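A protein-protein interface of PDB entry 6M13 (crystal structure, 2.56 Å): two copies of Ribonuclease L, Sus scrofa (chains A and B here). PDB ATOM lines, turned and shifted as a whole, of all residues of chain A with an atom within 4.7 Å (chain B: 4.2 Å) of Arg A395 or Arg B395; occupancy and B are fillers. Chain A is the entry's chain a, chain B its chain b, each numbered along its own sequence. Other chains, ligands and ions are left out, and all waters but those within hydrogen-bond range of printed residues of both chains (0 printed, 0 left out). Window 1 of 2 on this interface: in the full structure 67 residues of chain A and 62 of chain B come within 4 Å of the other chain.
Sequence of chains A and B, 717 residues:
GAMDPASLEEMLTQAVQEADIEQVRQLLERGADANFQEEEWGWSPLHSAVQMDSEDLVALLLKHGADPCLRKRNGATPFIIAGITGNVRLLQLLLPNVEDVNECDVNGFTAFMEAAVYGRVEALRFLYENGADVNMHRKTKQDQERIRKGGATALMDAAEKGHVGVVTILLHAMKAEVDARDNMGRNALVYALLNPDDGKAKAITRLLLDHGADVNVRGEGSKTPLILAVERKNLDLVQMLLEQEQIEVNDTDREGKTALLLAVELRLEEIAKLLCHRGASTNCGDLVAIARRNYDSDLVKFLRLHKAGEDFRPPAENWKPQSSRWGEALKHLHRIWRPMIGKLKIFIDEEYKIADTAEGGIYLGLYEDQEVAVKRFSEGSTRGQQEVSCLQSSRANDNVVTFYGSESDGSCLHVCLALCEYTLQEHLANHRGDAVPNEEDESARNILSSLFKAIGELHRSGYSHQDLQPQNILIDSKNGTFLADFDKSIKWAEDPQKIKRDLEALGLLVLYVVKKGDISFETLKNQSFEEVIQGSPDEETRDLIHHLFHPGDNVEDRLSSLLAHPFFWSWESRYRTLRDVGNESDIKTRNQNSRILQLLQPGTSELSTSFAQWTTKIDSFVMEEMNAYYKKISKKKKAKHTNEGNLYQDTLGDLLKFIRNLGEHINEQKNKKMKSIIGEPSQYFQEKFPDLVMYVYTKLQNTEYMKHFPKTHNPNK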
ATOM      1  N   GLU A 368     -16.813 -23.191  -5.444  1.00  0.00           N
ATOM      2  CA  GLU A 368     -16.928 -22.171  -4.382  1.00  0.00           C
ATOM      3  C   GLU A 368     -18.016 -22.559  -3.397  1.00  0.00           C
ATOM      4  O   GLU A 368     -18.854 -21.748  -2.997  1.00  0.00           O
ATOM      5  CB  GLU A 368     -17.231 -20.795  -4.977  1.00  0.00           C
ATOM      6  CG  GLU A 368     -16.152 -20.247  -5.915  1.00  0.00           C
ATOM      7  CD  GLU A 368     -16.589 -19.020  -6.729  1.00  0.00           C
ATOM      8  OE1 GLU A 368     -17.825 -18.760  -6.886  1.00  0.00           O
ATOM      9  OE2 GLU A 368     -15.683 -18.304  -7.215  1.00  0.00           O
ATOM     10  N   LEU A 391     -20.364 -20.241 -23.758  1.00  0.00           N
ATOM     11  CA  LEU A 391     -20.840 -19.981 -22.416  1.00  0.00           C
ATOM     12  C   LEU A 391     -20.418 -18.597 -21.877  1.00  0.00           C
ATOM     13  O   LEU A 391     -21.229 -17.915 -21.240  1.00  0.00           O
ATOM     14  CB  LEU A 391     -20.362 -21.066 -21.453  1.00  0.00           C
ATOM     15  CG  LEU A 391     -21.111 -22.376 -21.583  1.00  0.00           C
ATOM     16  CD1 LEU A 391     -20.363 -23.440 -20.828  1.00  0.00           C
ATOM     17  CD2 LEU A 391     -22.542 -22.287 -21.081  1.00  0.00           C
ATOM     18  N   GLN A 392     -19.176 -18.188 -22.128  1.00  0.00           N
ATOM     19  CA  GLN A 392     -18.725 -16.913 -21.604  1.00  0.00           C
ATOM     20  C   GLN A 392     -19.366 -15.683 -22.299  1.00  0.00           C
ATOM     21  O   GLN A 392     -19.398 -14.611 -21.708  1.00  0.00           O
ATOM     22  CB  GLN A 392     -17.202 -16.884 -21.407  1.00  0.00           C
ATOM     23  CG  GLN A 392     -16.348 -16.904 -22.637  1.00  0.00           C
ATOM     24  CD  GLN A 392     -14.916 -17.293 -22.298  1.00  0.00           C
ATOM     25  OE1 GLN A 392     -14.063 -17.434 -23.195  1.00  0.00           O
ATOM     26  NE2 GLN A 392     -14.641 -17.490 -20.994  1.00  0.00           N
ATOM     27  N   SER A 393     -19.942 -15.867 -23.483  1.00  0.00           N
ATOM     28  CA  SER A 393     -20.718 -14.825 -24.146  1.00  0.00           C
ATOM     29  C   SER A 393     -22.219 -14.856 -23.825  1.00  0.00           C
ATOM     30  O   SER A 393     -22.984 -14.006 -24.343  1.00  0.00           O
ATOM     31  CB  SER A 393     -20.558 -14.931 -25.675  1.00  0.00           C
ATOM     32  OG  SER A 393     -19.210 -15.159 -26.028  1.00  0.00           O
ATOM     33  N   SER A 394     -22.650 -15.803 -22.993  1.00  0.00           N
ATOM     34  CA  SER A 394     -24.070 -16.064 -22.791  1.00  0.00           C
ATOM     35  C   SER A 394     -24.545 -15.743 -21.373  1.00  0.00           C
ATOM     36  O   SER A 394     -25.694 -15.953 -21.043  1.00  0.00           O
ATOM     37  CB  SER A 394     -24.362 -17.529 -23.130  1.00  0.00           C
ATOM     38  OG  SER A 394     -24.466 -17.665 -24.533  1.00  0.00           O
ATOM     39  N   ARG A 395     -23.677 -15.131 -20.589  1.00  0.00           N
ATOM     40  CA  ARG A 395     -23.936 -14.826 -19.201  1.00  0.00           C
ATOM     41  C   ARG A 395     -25.191 -13.967 -18.967  1.00  0.00           C
ATOM     42  O   ARG A 395     -25.826 -14.151 -17.968  1.00  0.00           O
ATOM     43  CB  ARG A 395     -22.675 -14.228 -18.571  1.00  0.00           C
ATOM     44  CG  ARG A 395     -21.450 -15.121 -18.768  1.00  0.00           C
ATOM     45  CD  ARG A 395     -20.256 -14.664 -17.945  1.00  0.00           C
ATOM     46  NE  ARG A 395     -20.137 -15.425 -16.702  1.00  0.00           N
ATOM     47  CZ  ARG A 395     -19.018 -16.016 -16.254  1.00  0.00           C
ATOM     48  NH1 ARG A 395     -17.850 -15.956 -16.919  1.00  0.00           N
ATOM     49  NH2 ARG A 395     -19.055 -16.675 -15.106  1.00  0.00           N
ATOM     50  N   ALA A 396     -25.557 -13.105 -19.907  1.00  0.00           N
ATOM     51  CA  ALA A 396     -26.845 -12.359 -19.891  1.00  0.00           C
ATOM     52  C   ALA A 396     -28.045 -13.071 -20.492  1.00  0.00           C
ATOM     53  O   ALA A 396     -29.138 -12.538 -20.464  1.00  0.00           O
ATOM     54  CB  ALA A 396     -26.689 -11.028 -20.626  1.00  0.00           C
ATOM     55  N   ASN A 397     -27.866 -14.231 -21.091  1.00  0.00           N
ATOM     56  CA  ASN A 397     -28.990 -14.984 -21.622  1.00  0.00           C
ATOM     57  C   ASN A 397     -29.652 -15.726 -20.432  1.00  0.00           C
ATOM     58  O   ASN A 397     -29.074 -16.695 -19.906  1.00  0.00           O
ATOM     59  CB  ASN A 397     -28.476 -15.999 -22.653  1.00  0.00           C
ATOM     60  CG  ASN A 397     -29.587 -16.609 -23.483  1.00  0.00           C
ATOM     61  OD1 ASN A 397     -30.741 -16.691 -23.042  1.00  0.00           O
ATOM     62  ND2 ASN A 397     -29.246 -17.041 -24.707  1.00  0.00           N
ATOM     63  N   THR A 402     -26.606 -21.431 -16.336  1.00  0.00           N
ATOM     64  CA  THR A 402     -25.660 -20.502 -15.735  1.00  0.00           C
ATOM     65  C   THR A 402     -24.261 -21.102 -15.713  1.00  0.00           C
ATOM     66  O   THR A 402     -24.095 -22.272 -15.404  1.00  0.00           O
ATOM     67  CB  THR A 402     -26.092 -20.121 -14.310  1.00  0.00           C
ATOM     68  OG1 THR A 402     -27.460 -19.675 -14.338  1.00  0.00           O
ATOM     69  CG2 THR A 402     -25.215 -19.031 -13.726  1.00  0.00           C
ATOM     70  N   PHE A 403     -23.273 -20.283 -16.055  1.00  0.00           N
ATOM     71  CA  PHE A 403     -21.896 -20.708 -16.168  1.00  0.00           C
ATOM     72  C   PHE A 403     -21.078 -20.169 -15.014  1.00  0.00           C
ATOM     73  O   PHE A 403     -20.796 -18.978 -14.969  1.00  0.00           O
ATOM     74  CB  PHE A 403     -21.315 -20.221 -17.492  1.00  0.00           C
ATOM     75  CG  PHE A 403     -19.850 -20.490 -17.658  1.00  0.00           C
ATOM     76  CD1 PHE A 403     -19.325 -21.728 -17.454  1.00  0.00           C
ATOM     77  CD2 PHE A 403     -19.002 -19.488 -18.071  1.00  0.00           C
ATOM     78  CE1 PHE A 403     -17.981 -21.980 -17.646  1.00  0.00           C
ATOM     79  CE2 PHE A 403     -17.648 -19.727 -18.270  1.00  0.00           C
ATOM     80  CZ  PHE A 403     -17.140 -20.980 -18.046  1.00  0.00           C
ATOM     81  N   TYR A 404     -20.644 -21.060 -14.127  1.00  0.00           N
ATOM     82  CA  TYR A 404     -19.859 -20.672 -12.960  1.00  0.00           C
ATOM     83  C   TYR A 404     -18.420 -20.377 -13.334  1.00  0.00           C
ATOM     84  O   TYR A 404     -17.893 -19.320 -13.021  1.00  0.00           O
ATOM     85  CB  TYR A 404     -19.935 -21.737 -11.867  1.00  0.00           C
ATOM     86  CG  TYR A 404     -21.266 -21.756 -11.126  1.00  0.00           C
ATOM     87  CD1 TYR A 404     -22.440 -22.138 -11.754  1.00  0.00           C
ATOM     88  CD2 TYR A 404     -21.335 -21.421  -9.796  1.00  0.00           C
ATOM     89  CE1 TYR A 404     -23.642 -22.167 -11.074  1.00  0.00           C
ATOM     90  CE2 TYR A 404     -22.536 -21.464  -9.111  1.00  0.00           C
ATOM     91  CZ  TYR A 404     -23.689 -21.818  -9.767  1.00  0.00           C
ATOM     92  OH  TYR A 404     -24.866 -21.850  -9.088  1.00  0.00           O
ATOM     93  N   GLU B 368     -12.077 -12.575 -18.583  1.00  0.00           N
ATOM     94  CA  GLU B 368     -12.154 -13.557 -19.705  1.00  0.00           C
ATOM     95  C   GLU B 368     -12.496 -12.843 -21.015  1.00  0.00           C
ATOM     96  O   GLU B 368     -13.367 -13.268 -21.780  1.00  0.00           O
ATOM     97  CB  GLU B 368     -13.227 -14.611 -19.422  1.00  0.00           C
ATOM     98  CG  GLU B 368     -13.044 -15.471 -18.176  1.00  0.00           C
ATOM     99  CD  GLU B 368     -14.333 -16.251 -17.793  1.00  0.00           C
ATOM    100  OE1 GLU B 368     -15.470 -15.845 -18.186  1.00  0.00           O
ATOM    101  OE2 GLU B 368     -14.235 -17.285 -17.082  1.00  0.00           O
ATOM    102  N   LEU B 391     -23.824 -12.538  -3.764  1.00  0.00           N
ATOM    103  CA  LEU B 391     -23.741 -12.739  -5.217  1.00  0.00           C
ATOM    104  C   LEU B 391     -23.678 -14.217  -5.633  1.00  0.00           C
ATOM    105  O   LEU B 391     -24.299 -14.607  -6.573  1.00  0.00           O
ATOM    106  CB  LEU B 391     -22.561 -11.971  -5.819  1.00  0.00           C
ATOM    107  CG  LEU B 391     -22.776 -10.458  -5.872  1.00  0.00           C
ATOM    108  CD1 LEU B 391     -21.442  -9.770  -6.166  1.00  0.00           C
ATOM    109  CD2 LEU B 391     -23.869 -10.077  -6.861  1.00  0.00           C
ATOM    110  N   GLN B 392     -22.928 -15.033  -4.928  1.00  0.00           N
ATOM    111  CA  GLN B 392     -22.821 -16.465  -5.245  1.00  0.00           C
ATOM    112  C   GLN B 392     -24.132 -17.252  -5.082  1.00  0.00           C
ATOM    113  O   GLN B 392     -24.359 -18.248  -5.770  1.00  0.00           O
ATOM    114  CB  GLN B 392     -21.764 -17.093  -4.361  1.00  0.00           C
ATOM    115  CG  GLN B 392     -20.326 -16.763  -4.752  1.00  0.00           C
ATOM    116  CD  GLN B 392     -19.314 -17.174  -3.677  1.00  0.00           C
ATOM    117  OE1 GLN B 392     -19.635 -17.223  -2.490  1.00  0.00           O
ATOM    118  NE2 GLN B 392     -18.090 -17.473  -4.093  1.00  0.00           N
ATOM    119  N   SER B 393     -25.014 -16.764  -4.215  1.00  0.00           N
ATOM    120  CA  SER B 393     -26.348 -17.357  -4.027  1.00  0.00           C
ATOM    121  C   SER B 393     -27.433 -16.745  -4.917  1.00  0.00           C
ATOM    122  O   SER B 393     -28.617 -17.074  -4.769  1.00  0.00           O
ATOM    123  CB  SER B 393     -26.771 -17.213  -2.570  1.00  0.00           C
ATOM    124  OG  SER B 393     -25.703 -17.523  -1.682  1.00  0.00           O
ATOM    125  N   SER B 394     -27.048 -15.837  -5.816  1.00  0.00           N
ATOM    126  CA  SER B 394     -27.992 -15.098  -6.645  1.00  0.00           C
ATOM    127  C   SER B 394     -27.793 -15.337  -8.116  1.00  0.00           C
ATOM    128  O   SER B 394     -28.500 -14.748  -8.910  1.00  0.00           O
ATOM    129  CB  SER B 394     -27.918 -13.621  -6.289  1.00  0.00           C
ATOM    130  OG  SER B 394     -28.267 -13.557  -4.919  1.00  0.00           O
ATOM    131  N   ARG B 395     -26.942 -16.282  -8.479  1.00  0.00           N
ATOM    132  CA  ARG B 395     -26.636 -16.541  -9.894  1.00  0.00           C
ATOM    133  C   ARG B 395     -27.868 -16.934 -10.734  1.00  0.00           C
ATOM    134  O   ARG B 395     -27.893 -16.632 -11.897  1.00  0.00           O
ATOM    135  CB  ARG B 395     -25.529 -17.569 -10.013  1.00  0.00           C
ATOM    136  CG  ARG B 395     -24.285 -17.179  -9.225  1.00  0.00           C
ATOM    137  CD  ARG B 395     -23.115 -18.135  -9.427  1.00  0.00           C
ATOM    138  NE  ARG B 395     -22.281 -17.644 -10.526  1.00  0.00           N
ATOM    139  CZ  ARG B 395     -20.960 -17.523 -10.521  1.00  0.00           C
ATOM    140  NH1 ARG B 395     -20.213 -17.943  -9.496  1.00  0.00           N
ATOM    141  NH2 ARG B 395     -20.386 -17.005 -11.603  1.00  0.00           N
ATOM    142  N   ALA B 396     -28.902 -17.521 -10.124  1.00  0.00           N
ATOM    143  CA  ALA B 396     -30.206 -17.769 -10.780  1.00  0.00           C
ATOM    144  C   ALA B 396     -31.193 -16.609 -10.749  1.00  0.00           C
ATOM    145  O   ALA B 396     -32.249 -16.685 -11.389  1.00  0.00           O
ATOM    146  CB  ALA B 396     -30.887 -18.968 -10.143  1.00  0.00           C
ATOM    147  N   ASN B 397     -30.900 -15.551 -10.005  1.00  0.00           N
ATOM    148  CA  ASN B 397     -31.794 -14.404  -9.956  1.00  0.00           C
ATOM    149  C   ASN B 397     -31.579 -13.563 -11.195  1.00  0.00           C
ATOM    150  O   ASN B 397     -30.552 -12.924 -11.345  1.00  0.00           O
ATOM    151  CB  ASN B 397     -31.495 -13.605  -8.696  1.00  0.00           C
ATOM    152  CG  ASN B 397     -32.588 -12.607  -8.344  1.00  0.00           C
ATOM    153  OD1 ASN B 397     -33.349 -12.162  -9.203  1.00  0.00           O
ATOM    154  ND2 ASN B 397     -32.668 -12.272  -7.050  1.00  0.00           N
ATOM    155  N   THR B 402     -25.352  -9.596 -13.024  1.00  0.00           N
ATOM    156  CA  THR B 402     -24.669 -10.871 -13.251  1.00  0.00           C
ATOM    157  C   THR B 402     -23.294 -10.847 -12.621  1.00  0.00           C
ATOM    158  O   THR B 402     -22.580  -9.844 -12.724  1.00  0.00           O
ATOM    159  CB  THR B 402     -24.562 -11.186 -14.754  1.00  0.00           C
ATOM    160  OG1 THR B 402     -25.859 -11.084 -15.356  1.00  0.00           O
ATOM    161  CG2 THR B 402     -24.042 -12.591 -14.973  1.00  0.00           C
ATOM    162  N   PHE B 403     -22.939 -11.942 -11.962  1.00  0.00           N
ATOM    163  CA  PHE B 403     -21.691 -12.066 -11.256  1.00  0.00           C
ATOM    164  C   PHE B 403     -20.747 -12.977 -12.027  1.00  0.00           C
ATOM    165  O   PHE B 403     -20.948 -14.186 -12.075  1.00  0.00           O
ATOM    166  CB  PHE B 403     -21.957 -12.660  -9.878  1.00  0.00           C
ATOM    167  CG  PHE B 403     -20.719 -12.965  -9.092  1.00  0.00           C
ATOM    168  CD1 PHE B 403     -19.759 -12.025  -8.916  1.00  0.00           C
ATOM    169  CD2 PHE B 403     -20.562 -14.180  -8.475  1.00  0.00           C
ATOM    170  CE1 PHE B 403     -18.621 -12.298  -8.159  1.00  0.00           C
ATOM    171  CE2 PHE B 403     -19.429 -14.460  -7.723  1.00  0.00           C
ATOM    172  CZ  PHE B 403     -18.457 -13.526  -7.578  1.00  0.00           C
ATOM    173  N   TYR B 404     -19.679 -12.396 -12.560  1.00  0.00           N
ATOM    174  CA  TYR B 404     -18.695 -13.125 -13.333  1.00  0.00           C
ATOM    175  C   TYR B 404     -17.774 -13.892 -12.405  1.00  0.00           C
ATOM    176  O   TYR B 404     -17.583 -15.091 -12.583  1.00  0.00           O
ATOM    177  CB  TYR B 404     -17.895 -12.168 -14.235  1.00  0.00           C
ATOM    178  CG  TYR B 404     -18.662 -11.686 -15.459  1.00  0.00           C
ATOM    179  CD1 TYR B 404     -19.763 -10.865 -15.339  1.00  0.00           C
ATOM    180  CD2 TYR B 404     -18.282 -12.049 -16.728  1.00  0.00           C
ATOM    181  CE1 TYR B 404     -20.463 -10.421 -16.449  1.00  0.00           C
ATOM    182  CE2 TYR B 404     -18.983 -11.618 -17.837  1.00  0.00           C
ATOM    183  CZ  TYR B 404     -20.068 -10.813 -17.691  1.00  0.00           C
ATOM    184  OH  TYR B 404     -20.786 -10.395 -18.775  1.00  0.00           O
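Among the printed residues, merely in contact across the chains: Tyr A404 with Arg B395 (3.4 Å), Arg A395 with Arg B395 (3.8 Å), Arg A395 with Thr B402 (3.8 Å), Phe A403 with Arg B395 (3.9 Å) and Thr A402 with Arg B395 (3.9 Å).
Printed residues of chain B that touch a printed residue of chain A: Glu B368, Gln B392, Arg B395, Thr B402 and Tyr B404. Hydrophobic or aromatic side chains of chain B within 4 Å of the printed part of chain A: Tyr B404. Along chain B the printed residues that touch a printed residue of chain A span positions 368 to 404. Of the 11 printed residues of chain A, 6 touch a printed residue of chain B. Hydrophobic or aromatic side chains of chain A that line the printed part of chain B: Tyr A404.
The guanidinium group of Arg B395 is in hydrogen-bond range of the backbone carbonyl oxygen of Phe B403 (2.9 Å). The backbone carbonyl oxygen of Phe A403 lies within hydrogen-bond range of the guanidinium group of Arg A395 (2.9 Å).
Arg A395 touches just these residues of chain B: Glu B368, Arg B395, Thr B402 and Tyr B404. Of chain A, only Glu A368, Arg A395, Thr A402, Phe A403 and Tyr A404 come within 4 Å of Arg B395. Printed residues of chain A within 4 Å of Glu B368: Gln A392 and Arg A395. Printed residues of chain B within 4 Å of Gln A392: Glu B368. Ala A396 touches none of the printed residues of chain B. The nearest printed residue of chain A that does not touch Arg B395 is Asn A397 (8.1 Å).
NH1 of Arg A395 is in salt-bridge range of OE1 of Glu B368 (2.7 Å). NH2 of Arg A395 sits at hydrogen-bond distance from O of Tyr B404, 3.3 Å away. The side-chain carboxylate (OE1) of Glu A368 is in salt-bridge range of the guanidinium group (NH1) of Arg B395 (3.6 Å). NE2 of Gln B392 is in hydrogen-bond range of OE1 of Glu A368, 3.1 Å away. The side-chain carboxylate (OE1) of Glu B368 sits at hydrogen-bond distance from the side-chain amide nitrogen (NE2) of Gln A392 (3.4 Å).
Glu A368 touches Gln B392, and with the chains exchanged Gln A392 touches Glu B368. Arg B395 touches its own counterpart, Arg A395. Arg A395 touches Tyr B404, and with the chains exchanged Tyr A404 touches Arg B395. Phe A403 touches Arg B395, but with the chains exchanged Arg A395 does not touch Phe B403 (4.4 Å). Of the 10 pairs that touch across the chains among the printed residues, 9 have their exchanged pair printed and touching as well.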
